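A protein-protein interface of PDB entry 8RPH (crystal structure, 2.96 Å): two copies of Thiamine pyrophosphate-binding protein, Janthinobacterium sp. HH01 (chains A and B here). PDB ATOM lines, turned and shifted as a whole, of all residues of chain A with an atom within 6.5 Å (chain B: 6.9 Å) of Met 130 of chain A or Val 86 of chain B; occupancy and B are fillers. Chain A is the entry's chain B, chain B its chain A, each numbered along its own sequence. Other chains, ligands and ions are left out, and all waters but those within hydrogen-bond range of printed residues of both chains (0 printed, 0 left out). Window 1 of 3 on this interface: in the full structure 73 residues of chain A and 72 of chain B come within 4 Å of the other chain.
OG1 of Thr 83 of chain A lies within hydrogen-bond range of OG1 of Thr 87 of chain B, at 2.9 Å. NE2 of Gln 129 of chain B is in hydrogen-bond range of O of Gln 129 of chain A.
The backbone NH (N) of Thr 83 of chain A lies close to the side-chain hydroxyl (OH) of Tyr 125 of chain A, 3.3 Å away. OG of Ser 91 of chain B sits at hydrogen-bond distance from O of Thr 87 of chain B (3.2 Å). The side-chain hydroxyl (OH) of Tyr 125 of chain B sits close to the side-chain sulfur (SD) of Met 130 of chain B (3.6 Å). OD1 of Asp 126 of chain A lies within hydrogen-bond range of N of Gln 129 of chain A (2.7 Å). The side-chain sulfur (SD) of Met 130 of chain A lies within hydrogen-bond range of the side-chain hydroxyl (OH) of Tyr 125 of chain A (3.7 Å).
CG1 of Val 86 of chain A touches SD of Met 130 of chain B, at 3.5 Å. Gln 129 of chain A touches Glu 132 of chain B (NE2 to CB, 3.9 Å). Arg 133 of chain B touches Gln 129 of chain A (CG to CD, 3.4 Å). SD of Met 130 of chain A touches CG1 of Val 86 of chain B, 3.4 Å away. CG of Met 130 of chain A touches O of Met 130 of chain B, 3.6 Å away. Met 130 of chain A touches Val 134 of chain B (CE to CG2, 3.99 Å). Arg 133 of chain A touches Gln 129 of chain B.
Of the printed residues of chain B, Met 130 of chain A touches Val 86 (3.4 Å), Met 130 (3.6 Å) and Val 134 (3.99 Å). Val 86 of chain B touches just one residue of chain A: Met 130 (3.4 Å). Val 90 of chain B touches none of the printed residues of chain A. Of the printed residues of chain A, Met 130 of chain B touches Val 86 and Met 130. Of the printed residues of chain A, Val 134 of chain B touches Met 130 (3.99 Å). The nearest residue of chain A that does not touch Val 86 of chain B is Thr 83 of chain A (4.4 Å).
Printed residues of chain B that touch a printed residue of chain A: Val 86, Thr 87, Gln 129, Met 130, Glu 132, Arg 133 and Val 134. Hydrophobic or aromatic side chains of chain B within 4 Å of the printed part of chain A: Val 86, Met 130 and Val 134. Hydrophobic or aromatic side chains of chain A within 4 Å of the printed part of chain B: Val 86 and Met 130.
Gln 129 of chain B touches its own counterpart, Gln 129 of chain A. Gln 129 of chain A touches Glu 132 of chain B, but with the chains exchanged Glu 132 of chain A does not touch Gln 129 of chain B (4.1 Å). Gln 129 of chain A touches Arg 133 of chain B, and with the chains exchanged Arg 133 of chain A touches Gln 129 of chain B. Met 130 of chain A touches its own counterpart, Met 130 of chain B.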
ATOM      1  N   SER A  82     -21.281   6.364 -16.933  1.00  0.00           N
ATOM      2  CA  SER A  82     -20.317   6.777 -15.921  1.00  0.00           C
ATOM      3  C   SER A  82     -20.671   6.234 -14.540  1.00  0.00           C
ATOM      4  O   SER A  82     -19.788   5.756 -13.820  1.00  0.00           O
ATOM      5  CB  SER A  82     -20.229   8.301 -15.887  1.00  0.00           C
ATOM      6  OG  SER A  82     -19.826   8.804 -17.150  1.00  0.00           O
ATOM      7  N   THR A  83     -21.950   6.287 -14.154  1.00  0.00           N
ATOM      8  CA  THR A  83     -22.332   5.794 -12.833  1.00  0.00           C
ATOM      9  C   THR A  83     -22.094   4.295 -12.703  1.00  0.00           C
ATOM     10  O   THR A  83     -21.854   3.799 -11.596  1.00  0.00           O
ATOM     11  CB  THR A  83     -23.802   6.111 -12.543  1.00  0.00           C
ATOM     12  OG1 THR A  83     -24.640   5.460 -13.507  1.00  0.00           O
ATOM     13  CG2 THR A  83     -24.053   7.609 -12.582  1.00  0.00           C
ATOM     14  N   VAL A  86     -18.517   3.480 -11.213  1.00  0.00           N
ATOM     15  CA  VAL A  86     -18.065   4.010  -9.928  1.00  0.00           C
ATOM     16  C   VAL A  86     -17.457   2.907  -9.067  1.00  0.00           C
ATOM     17  O   VAL A  86     -16.452   3.123  -8.381  1.00  0.00           O
ATOM     18  CB  VAL A  86     -19.227   4.719  -9.207  1.00  0.00           C
ATOM     19  CG1 VAL A  86     -18.790   5.195  -7.829  1.00  0.00           C
ATOM     20  CG2 VAL A  86     -19.721   5.889 -10.039  1.00  0.00           C
ATOM     21  N   TYR A 125     -24.779  14.383 -15.763  1.00  0.00           N
ATOM     22  CA  TYR A 125     -24.579  14.768 -14.374  1.00  0.00           C
ATOM     23  C   TYR A 125     -23.092  15.008 -14.147  1.00  0.00           C
ATOM     24  O   TYR A 125     -22.254  14.683 -14.992  1.00  0.00           O
ATOM     25  CB  TYR A 125     -25.102  13.695 -13.419  1.00  0.00           C
ATOM     26  CG  TYR A 125     -24.157  12.527 -13.279  1.00  0.00           C
ATOM     27  CD1 TYR A 125     -24.056  11.568 -14.277  1.00  0.00           C
ATOM     28  CD2 TYR A 125     -23.359  12.390 -12.155  1.00  0.00           C
ATOM     29  CE1 TYR A 125     -23.186  10.503 -14.154  1.00  0.00           C
ATOM     30  CE2 TYR A 125     -22.490  11.329 -12.022  1.00  0.00           C
ATOM     31  CZ  TYR A 125     -22.405  10.391 -13.023  1.00  0.00           C
ATOM     32  OH  TYR A 125     -21.536   9.334 -12.887  1.00  0.00           O
ATOM     33  N   ASP A 126     -22.776  15.574 -12.984  1.00  0.00           N
ATOM     34  CA  ASP A 126     -21.397  15.888 -12.613  1.00  0.00           C
ATOM     35  C   ASP A 126     -20.700  14.593 -12.227  1.00  0.00           C
ATOM     36  O   ASP A 126     -20.675  14.197 -11.061  1.00  0.00           O
ATOM     37  CB  ASP A 126     -21.360  16.891 -11.469  1.00  0.00           C
ATOM     38  CG  ASP A 126     -19.972  17.449 -11.226  1.00  0.00           C
ATOM     39  OD1 ASP A 126     -18.986  16.699 -11.392  1.00  0.00           O
ATOM     40  OD2 ASP A 126     -19.867  18.643 -10.872  1.00  0.00           O
ATOM     41  N   SER A 127     -20.118  13.924 -13.223  1.00  0.00           N
ATOM     42  CA  SER A 127     -19.412  12.679 -12.958  1.00  0.00           C
ATOM     43  C   SER A 127     -18.099  12.907 -12.218  1.00  0.00           C
ATOM     44  O   SER A 127     -17.539  11.953 -11.668  1.00  0.00           O
ATOM     45  CB  SER A 127     -19.161  11.933 -14.267  1.00  0.00           C
ATOM     46  OG  SER A 127     -18.240  12.627 -15.089  1.00  0.00           O
ATOM     47  N   CYS A 128     -17.601  14.143 -12.178  1.00  0.00           N
ATOM     48  CA  CYS A 128     -16.392  14.429 -11.415  1.00  0.00           C
ATOM     49  C   CYS A 128     -16.686  14.528  -9.924  1.00  0.00           C
ATOM     50  O   CYS A 128     -15.900  14.051  -9.097  1.00  0.00           O
ATOM     51  CB  CYS A 128     -15.750  15.723 -11.914  1.00  0.00           C
ATOM     52  SG  CYS A 128     -14.983  15.590 -13.540  1.00  0.00           S
ATOM     53  N   GLN A 129     -17.812  15.147  -9.564  1.00  0.00           N
ATOM     54  CA  GLN A 129     -18.173  15.267  -8.158  1.00  0.00           C
ATOM     55  C   GLN A 129     -18.444  13.905  -7.530  1.00  0.00           C
ATOM     56  O   GLN A 129     -18.185  13.711  -6.337  1.00  0.00           O
ATOM     57  CB  GLN A 129     -19.396  16.176  -8.016  1.00  0.00           C
ATOM     58  CG  GLN A 129     -19.871  16.376  -6.586  1.00  0.00           C
ATOM     59  CD  GLN A 129     -20.783  15.268  -6.102  1.00  0.00           C
ATOM     60  OE1 GLN A 129     -21.400  14.561  -6.899  1.00  0.00           O
ATOM     61  NE2 GLN A 129     -20.870  15.107  -4.787  1.00  0.00           N
ATOM     62  N   MET A 130     -18.956  12.951  -8.311  1.00  0.00           N
ATOM     63  CA  MET A 130     -19.340  11.664  -7.738  1.00  0.00           C
ATOM     64  C   MET A 130     -18.129  10.856  -7.284  1.00  0.00           C
ATOM     65  O   MET A 130     -18.217  10.119  -6.296  1.00  0.00           O
ATOM     66  CB  MET A 130     -20.165  10.869  -8.750  1.00  0.00           C
ATOM     67  CG  MET A 130     -20.720   9.566  -8.201  1.00  0.00           C
ATOM     68  SD  MET A 130     -21.996   8.844  -9.255  1.00  0.00           S
ATOM     69  CE  MET A 130     -23.355   9.988  -9.023  1.00  0.00           C
ATOM     70  N   VAL A 131     -16.998  10.981  -7.975  1.00  0.00           N
ATOM     71  CA  VAL A 131     -15.786  10.247  -7.631  1.00  0.00           C
ATOM     72  C   VAL A 131     -14.740  11.169  -6.997  1.00  0.00           C
ATOM     73  O   VAL A 131     -13.565  10.817  -6.924  1.00  0.00           O
ATOM     74  CB  VAL A 131     -15.217   9.512  -8.857  1.00  0.00           C
ATOM     75  CG1 VAL A 131     -16.249   8.541  -9.415  1.00  0.00           C
ATOM     76  CG2 VAL A 131     -14.789  10.500  -9.933  1.00  0.00           C
ATOM     77  N   GLU A 132     -15.166  12.346  -6.526  1.00  0.00           N
ATOM     78  CA  GLU A 132     -14.242  13.311  -5.934  1.00  0.00           C
ATOM     79  C   GLU A 132     -13.446  12.713  -4.777  1.00  0.00           C
ATOM     80  O   GLU A 132     -12.278  13.066  -4.580  1.00  0.00           O
ATOM     81  CB  GLU A 132     -15.021  14.534  -5.447  1.00  0.00           C
ATOM     82  CG  GLU A 132     -14.562  15.867  -6.010  1.00  0.00           C
ATOM     83  CD  GLU A 132     -15.517  16.993  -5.656  1.00  0.00           C
ATOM     84  OE1 GLU A 132     -16.119  16.935  -4.562  1.00  0.00           O
ATOM     85  OE2 GLU A 132     -15.675  17.927  -6.472  1.00  0.00           O
ATOM     86  N   ARG A 133     -14.058  11.826  -3.993  1.00  0.00           N
ATOM     87  CA  ARG A 133     -13.436  11.284  -2.792  1.00  0.00           C
ATOM     88  C   ARG A 133     -12.935   9.856  -2.980  1.00  0.00           C
ATOM     89  O   ARG A 133     -12.560   9.210  -1.996  1.00  0.00           O
ATOM     90  CB  ARG A 133     -14.421  11.334  -1.618  1.00  0.00           C
ATOM     91  CG  ARG A 133     -15.087  12.691  -1.387  1.00  0.00           C
ATOM     92  CD  ARG A 133     -14.097  13.770  -0.960  1.00  0.00           C
ATOM     93  NE  ARG A 133     -13.585  13.572   0.392  1.00  0.00           N
ATOM     94  CZ  ARG A 133     -12.701  14.367   0.981  1.00  0.00           C
ATOM     95  NH1 ARG A 133     -12.193  15.419   0.357  1.00  0.00           N
ATOM     96  NH2 ARG A 133     -12.316  14.104   2.227  1.00  0.00           N
ATOM     97  N   VAL A 134     -12.921   9.349  -4.212  1.00  0.00           N
ATOM     98  CA  VAL A 134     -12.453   7.993  -4.483  1.00  0.00           C
ATOM     99  C   VAL A 134     -11.591   7.978  -5.741  1.00  0.00           C
ATOM    100  O   VAL A 134     -11.568   6.990  -6.483  1.00  0.00           O
ATOM    101  CB  VAL A 134     -13.636   7.017  -4.615  1.00  0.00           C
ATOM    102  CG1 VAL A 134     -14.297   6.816  -3.266  1.00  0.00           C
ATOM    103  CG2 VAL A 134     -14.644   7.525  -5.637  1.00  0.00           C
ATOM    104  N   GLU B  54     -26.742  -4.913  -6.574  1.00  0.00           N
ATOM    105  CA  GLU B  54     -27.444  -3.866  -5.842  1.00  0.00           C
ATOM    106  C   GLU B  54     -28.109  -2.868  -6.782  1.00  0.00           C
ATOM    107  O   GLU B  54     -29.123  -2.256  -6.424  1.00  0.00           O
ATOM    108  CB  GLU B  54     -26.480  -3.143  -4.895  1.00  0.00           C
ATOM    109  CG  GLU B  54     -26.082  -3.947  -3.655  1.00  0.00           C
ATOM    110  CD  GLU B  54     -24.989  -4.964  -3.926  1.00  0.00           C
ATOM    111  OE1 GLU B  54     -24.622  -5.144  -5.107  1.00  0.00           O
ATOM    112  OE2 GLU B  54     -24.500  -5.583  -2.954  1.00  0.00           O
ATOM    113  N   GLN B  55     -27.560  -2.692  -7.985  1.00  0.00           N
ATOM    114  CA  GLN B  55     -28.171  -1.791  -8.958  1.00  0.00           C
ATOM    115  C   GLN B  55     -29.633  -2.151  -9.194  1.00  0.00           C
ATOM    116  O   GLN B  55     -30.507  -1.276  -9.223  1.00  0.00           O
ATOM    117  CB  GLN B  55     -27.386  -1.831 -10.273  1.00  0.00           C
ATOM    118  CG  GLN B  55     -28.005  -1.005 -11.398  1.00  0.00           C
ATOM    119  CD  GLN B  55     -27.133  -0.938 -12.643  1.00  0.00           C
ATOM    120  OE1 GLN B  55     -27.605  -1.175 -13.756  1.00  0.00           O
ATOM    121  NE2 GLN B  55     -25.861  -0.597 -12.461  1.00  0.00           N
ATOM    122  N   CYS B  58     -32.000  -0.803  -6.421  1.00  0.00           N
ATOM    123  CA  CYS B  58     -32.340   0.610  -6.468  1.00  0.00           C
ATOM    124  C   CYS B  58     -33.188   0.963  -7.680  1.00  0.00           C
ATOM    125  O   CYS B  58     -33.747   2.066  -7.723  1.00  0.00           O
ATOM    126  CB  CYS B  58     -31.058   1.442  -6.452  1.00  0.00           C
ATOM    127  SG  CYS B  58     -30.000   1.092  -5.031  1.00  0.00           S
ATOM    128  N   LEU B  76     -28.845  -1.851   1.241  1.00  0.00           N
ATOM    129  CA  LEU B  76     -27.485  -2.012   0.751  1.00  0.00           C
ATOM    130  C   LEU B  76     -26.516  -2.134   1.916  1.00  0.00           C
ATOM    131  O   LEU B  76     -26.786  -1.676   3.030  1.00  0.00           O
ATOM    132  CB  LEU B  76     -27.082  -0.827  -0.127  1.00  0.00           C
ATOM    133  CG  LEU B  76     -28.102  -0.394  -1.175  1.00  0.00           C
ATOM    134  CD1 LEU B  76     -27.506   0.715  -2.019  1.00  0.00           C
ATOM    135  CD2 LEU B  76     -28.540  -1.567  -2.037  1.00  0.00           C
ATOM    136  N   GLY B  81     -21.476  -2.712  -1.872  1.00  0.00           N
ATOM    137  CA  GLY B  81     -22.925  -2.765  -1.767  1.00  0.00           C
ATOM    138  C   GLY B  81     -23.574  -1.425  -2.049  1.00  0.00           C
ATOM    139  O   GLY B  81     -24.610  -1.351  -2.712  1.00  0.00           O
ATOM    140  N   SER B  82     -22.965  -0.345  -1.560  1.00  0.00           N
ATOM    141  CA  SER B  82     -23.519   0.985  -1.773  1.00  0.00           C
ATOM    142  C   SER B  82     -23.208   1.501  -3.173  1.00  0.00           C
ATOM    143  O   SER B  82     -24.091   2.034  -3.854  1.00  0.00           O
ATOM    144  CB  SER B  82     -22.980   1.948  -0.713  1.00  0.00           C
ATOM    145  OG  SER B  82     -23.354   1.530   0.590  1.00  0.00           O
ATOM    146  N   THR B  83     -21.961   1.348  -3.624  1.00  0.00           N
ATOM    147  CA  THR B  83     -21.582   1.891  -4.927  1.00  0.00           C
ATOM    148  C   THR B  83     -22.381   1.243  -6.053  1.00  0.00           C
ATOM    149  O   THR B  83     -22.728   1.905  -7.037  1.00  0.00           O
ATOM    150  CB  THR B  83     -20.084   1.703  -5.169  1.00  0.00           C
ATOM    151  OG1 THR B  83     -19.770   0.305  -5.204  1.00  0.00           O
ATOM    152  CG2 THR B  83     -19.265   2.381  -4.077  1.00  0.00           C
ATOM    153  N   ASN B  84     -22.685  -0.051  -5.927  1.00  0.00           N
ATOM    154  CA  ASN B  84     -23.411  -0.747  -6.982  1.00  0.00           C
ATOM    155  C   ASN B  84     -24.827  -0.225  -7.180  1.00  0.00           C
ATOM    156  O   ASN B  84     -25.443  -0.542  -8.203  1.00  0.00           O
ATOM    157  CB  ASN B  84     -23.470  -2.248  -6.687  1.00  0.00           C
ATOM    158  CG  ASN B  84     -22.192  -2.971  -7.047  1.00  0.00           C
ATOM    159  OD1 ASN B  84     -21.329  -2.434  -7.739  1.00  0.00           O
ATOM    160  ND2 ASN B  84     -22.070  -4.208  -6.589  1.00  0.00           N
ATOM    161  N   GLY B  85     -25.361   0.552  -6.243  1.00  0.00           N
ATOM    162  CA  GLY B  85     -26.699   1.087  -6.365  1.00  0.00           C
ATOM    163  C   GLY B  85     -26.796   2.504  -6.886  1.00  0.00           C
ATOM    164  O   GLY B  85     -27.909   3.021  -7.025  1.00  0.00           O
ATOM    165  N   VAL B  86     -25.670   3.149  -7.194  1.00  0.00           N
ATOM    166  CA  VAL B  86     -25.700   4.572  -7.527  1.00  0.00           C
ATOM    167  C   VAL B  86     -26.489   4.814  -8.809  1.00  0.00           C
ATOM    168  O   VAL B  86     -27.234   5.795  -8.917  1.00  0.00           O
ATOM    169  CB  VAL B  86     -24.267   5.125  -7.623  1.00  0.00           C
ATOM    170  CG1 VAL B  86     -24.274   6.549  -8.140  1.00  0.00           C
ATOM    171  CG2 VAL B  86     -23.592   5.070  -6.259  1.00  0.00           C
ATOM    172  N   THR B  87     -26.344   3.930  -9.800  1.00  0.00           N
ATOM    173  CA  THR B  87     -27.088   4.100 -11.046  1.00  0.00           C
ATOM    174  C   THR B  87     -28.588   4.167 -10.787  1.00  0.00           C
ATOM    175  O   THR B  87     -29.287   5.007 -11.364  1.00  0.00           O
ATOM    176  CB  THR B  87     -26.773   2.960 -12.014  1.00  0.00           C
ATOM    177  OG1 THR B  87     -25.364   2.916 -12.264  1.00  0.00           O
ATOM    178  CG2 THR B  87     -27.518   3.151 -13.335  1.00  0.00           C
ATOM    179  N   GLY B  88     -29.099   3.288  -9.921  1.00  0.00           N
ATOM    180  CA  GLY B  88     -30.522   3.302  -9.625  1.00  0.00           C
ATOM    181  C   GLY B  88     -30.966   4.587  -8.957  1.00  0.00           C
ATOM    182  O   GLY B  88     -32.057   5.095  -9.226  1.00  0.00           O
ATOM    183  N   VAL B  89     -30.128   5.134  -8.075  1.00  0.00           N
ATOM    184  CA  VAL B  89     -30.472   6.387  -7.412  1.00  0.00           C
ATOM    185  C   VAL B  89     -30.610   7.505  -8.439  1.00  0.00           C
ATOM    186  O   VAL B  89     -31.566   8.289  -8.400  1.00  0.00           O
ATOM    187  CB  VAL B  89     -29.426   6.730  -6.335  1.00  0.00           C
ATOM    188  CG1 VAL B  89     -29.727   8.082  -5.699  1.00  0.00           C
ATOM    189  CG2 VAL B  89     -29.386   5.642  -5.273  1.00  0.00           C
ATOM    190  N   VAL B  90     -29.664   7.589  -9.379  1.00  0.00           N
ATOM    191  CA  VAL B  90     -29.682   8.678 -10.353  1.00  0.00           C
ATOM    192  C   VAL B  90     -30.929   8.593 -11.224  1.00  0.00           C
ATOM    193  O   VAL B  90     -31.499   9.618 -11.617  1.00  0.00           O
ATOM    194  CB  VAL B  90     -28.394   8.659 -11.200  1.00  0.00           C
ATOM    195  CG1 VAL B  90     -28.408   9.782 -12.227  1.00  0.00           C
ATOM    196  CG2 VAL B  90     -27.172   8.789 -10.310  1.00  0.00           C
ATOM    197  N   SER B  91     -31.376   7.374 -11.536  1.00  0.00           N
ATOM    198  CA  SER B  91     -32.539   7.225 -12.406  1.00  0.00           C
ATOM    199  C   SER B  91     -33.827   7.626 -11.690  1.00  0.00           C
ATOM    200  O   SER B  91     -34.706   8.254 -12.294  1.00  0.00           O
ATOM    201  CB  SER B  91     -32.624   5.791 -12.934  1.00  0.00           C
ATOM    202  OG  SER B  91     -32.462   4.837 -11.902  1.00  0.00           O
ATOM    203  N   TYR B 125     -16.757   3.780   2.920  1.00  0.00           N
ATOM    204  CA  TYR B 125     -16.527   5.075   2.293  1.00  0.00           C
ATOM    205  C   TYR B 125     -17.730   5.961   2.599  1.00  0.00           C
ATOM    206  O   TYR B 125     -18.695   5.532   3.240  1.00  0.00           O
ATOM    207  CB  TYR B 125     -16.306   4.926   0.785  1.00  0.00           C
ATOM    208  CG  TYR B 125     -17.586   4.742   0.008  1.00  0.00           C
ATOM    209  CD1 TYR B 125     -18.293   3.548   0.068  1.00  0.00           C
ATOM    210  CD2 TYR B 125     -18.093   5.763  -0.782  1.00  0.00           C
ATOM    211  CE1 TYR B 125     -19.469   3.378  -0.639  1.00  0.00           C
ATOM    212  CE2 TYR B 125     -19.263   5.601  -1.492  1.00  0.00           C
ATOM    213  CZ  TYR B 125     -19.950   4.409  -1.416  1.00  0.00           C
ATOM    214  OH  TYR B 125     -21.120   4.247  -2.123  1.00  0.00           O
ATOM    215  N   SER B 127     -20.715   7.056   1.575  1.00  0.00           N
ATOM    216  CA  SER B 127     -21.820   6.816   0.655  1.00  0.00           C
ATOM    217  C   SER B 127     -22.761   8.011   0.554  1.00  0.00           C
ATOM    218  O   SER B 127     -23.471   8.141  -0.450  1.00  0.00           O
ATOM    219  CB  SER B 127     -22.602   5.576   1.092  1.00  0.00           C
ATOM    220  OG  SER B 127     -23.337   5.824   2.280  1.00  0.00           O
ATOM    221  N   GLN B 129     -21.805  11.340   0.547  1.00  0.00           N
ATOM    222  CA  GLN B 129     -21.215  12.312  -0.365  1.00  0.00           C
ATOM    223  C   GLN B 129     -21.360  11.877  -1.816  1.00  0.00           C
ATOM    224  O   GLN B 129     -21.455  12.722  -2.714  1.00  0.00           O
ATOM    225  CB  GLN B 129     -19.739  12.522  -0.018  1.00  0.00           C
ATOM    226  CG  GLN B 129     -19.016  13.510  -0.923  1.00  0.00           C
ATOM    227  CD  GLN B 129     -18.515  12.888  -2.214  1.00  0.00           C
ATOM    228  OE1 GLN B 129     -18.271  11.683  -2.286  1.00  0.00           O
ATOM    229  NE2 GLN B 129     -18.364  13.709  -3.246  1.00  0.00           N
ATOM    230  N   MET B 130     -21.377  10.568  -2.070  1.00  0.00           N
ATOM    231  CA  MET B 130     -21.380  10.089  -3.446  1.00  0.00           C
ATOM    232  C   MET B 130     -22.717  10.343  -4.132  1.00  0.00           C
ATOM    233  O   MET B 130     -22.754  10.555  -5.349  1.00  0.00           O
ATOM    234  CB  MET B 130     -21.036   8.603  -3.477  1.00  0.00           C
ATOM    235  CG  MET B 130     -20.950   8.021  -4.870  1.00  0.00           C
ATOM    236  SD  MET B 130     -20.169   6.400  -4.878  1.00  0.00           S
ATOM    237  CE  MET B 130     -18.468   6.837  -4.522  1.00  0.00           C
ATOM    238  N   VAL B 131     -23.815  10.324  -3.382  1.00  0.00           N
ATOM    239  CA  VAL B 131     -25.133  10.631  -3.923  1.00  0.00           C
ATOM    240  C   VAL B 131     -25.597  12.025  -3.493  1.00  0.00           C
ATOM    241  O   VAL B 131     -26.791  12.318  -3.518  1.00  0.00           O
ATOM    242  CB  VAL B 131     -26.159   9.556  -3.537  1.00  0.00           C
ATOM    243  CG1 VAL B 131     -25.804   8.246  -4.203  1.00  0.00           C
ATOM    244  CG2 VAL B 131     -26.214   9.377  -2.029  1.00  0.00           C
ATOM    245  N   GLU B 132     -24.656  12.893  -3.119  1.00  0.00           N
ATOM    246  CA  GLU B 132     -24.995  14.204  -2.579  1.00  0.00           C
ATOM    247  C   GLU B 132     -25.682  15.089  -3.610  1.00  0.00           C
ATOM    248  O   GLU B 132     -26.486  15.955  -3.245  1.00  0.00           O
ATOM    249  CB  GLU B 132     -23.721  14.876  -2.076  1.00  0.00           C
ATOM    250  CG  GLU B 132     -23.886  15.724  -0.845  1.00  0.00           C
ATOM    251  CD  GLU B 132     -22.547  16.118  -0.255  1.00  0.00           C
ATOM    252  OE1 GLU B 132     -21.727  16.707  -0.995  1.00  0.00           O
ATOM    253  OE2 GLU B 132     -22.309  15.825   0.939  1.00  0.00           O
ATOM    254  N   ARG B 133     -25.376  14.899  -4.892  1.00  0.00           N
ATOM    255  CA  ARG B 133     -25.926  15.722  -5.959  1.00  0.00           C
ATOM    256  C   ARG B 133     -26.960  14.979  -6.799  1.00  0.00           C
ATOM    257  O   ARG B 133     -27.404  15.508  -7.824  1.00  0.00           O
ATOM    258  CB  ARG B 133     -24.795  16.234  -6.854  1.00  0.00           C
ATOM    259  CG  ARG B 133     -23.705  17.003  -6.109  1.00  0.00           C
ATOM    260  CD  ARG B 133     -24.214  18.310  -5.505  1.00  0.00           C
ATOM    261  NE  ARG B 133     -24.776  19.206  -6.510  1.00  0.00           N
ATOM    262  CZ  ARG B 133     -25.182  20.445  -6.268  1.00  0.00           C
ATOM    263  NH1 ARG B 133     -25.100  20.978  -5.058  1.00  0.00           N
ATOM    264  NH2 ARG B 133     -25.680  21.171  -7.265  1.00  0.00           N
ATOM    265  N   VAL B 134     -27.353  13.773  -6.394  1.00  0.00           N
ATOM    266  CA  VAL B 134     -28.346  12.999  -7.131  1.00  0.00           C
ATOM    267  C   VAL B 134     -29.321  12.349  -6.154  1.00  0.00           C
ATOM    268  O   VAL B 134     -29.780  11.223  -6.376  1.00  0.00           O
ATOM    269  CB  VAL B 134     -27.672  11.942  -8.029  1.00  0.00           C
ATOM    270  CG1 VAL B 134     -26.898  12.609  -9.159  1.00  0.00           C
ATOM    271  CG2 VAL B 134     -26.746  11.050  -7.214  1.00  0.00           C
ATOM    272  N   TRP B 167     -31.110   8.979   0.910  1.00  0.00           N
ATOM    273  CA  TRP B 167     -30.040   8.064   1.303  1.00  0.00           C
ATOM    274  C   TRP B 167     -29.815   8.184   2.804  1.00  0.00           C
ATOM    275  O   TRP B 167     -29.316   9.208   3.281  1.00  0.00           O
ATOM    276  CB  TRP B 167     -28.751   8.369   0.538  1.00  0.00           C
ATOM    277  CG  TRP B 167     -27.682   7.331   0.706  1.00  0.00           C
ATOM    278  CD1 TRP B 167     -26.864   7.158   1.788  1.00  0.00           C
ATOM    279  CD2 TRP B 167     -27.311   6.322  -0.242  1.00  0.00           C
ATOM    280  NE1 TRP B 167     -26.011   6.103   1.571  1.00  0.00           N
ATOM    281  CE2 TRP B 167     -26.265   5.573   0.333  1.00  0.00           C
ATOM    282  CE3 TRP B 167     -27.762   5.979  -1.520  1.00  0.00           C
ATOM    283  CZ2 TRP B 167     -25.665   4.501  -0.326  1.00  0.00           C
ATOM    284  CZ3 TRP B 167     -27.162   4.918  -2.173  1.00  0.00           C
ATOM    285  CH2 TRP B 167     -26.127   4.190  -1.575  1.00  0.00           C
ATOM    286  N   LEU B 432     -32.781   9.260 -16.982  1.00  0.00           N
ATOM    287  CA  LEU B 432     -31.412   8.793 -17.150  1.00  0.00           C
ATOM    288  C   LEU B 432     -31.237   7.920 -18.381  1.00  0.00           C
ATOM    289  O   LEU B 432     -30.145   7.892 -18.958  1.00  0.00           O
ATOM    290  CB  LEU B 432     -30.962   8.014 -15.907  1.00  0.00           C
ATOM    291  CG  LEU B 432     -29.491   7.594 -15.844  1.00  0.00           C
ATOM    292  CD1 LEU B 432     -28.559   8.800 -15.825  1.00  0.00           C
ATOM    293  CD2 LEU B 432     -29.254   6.725 -14.624  1.00  0.00           C
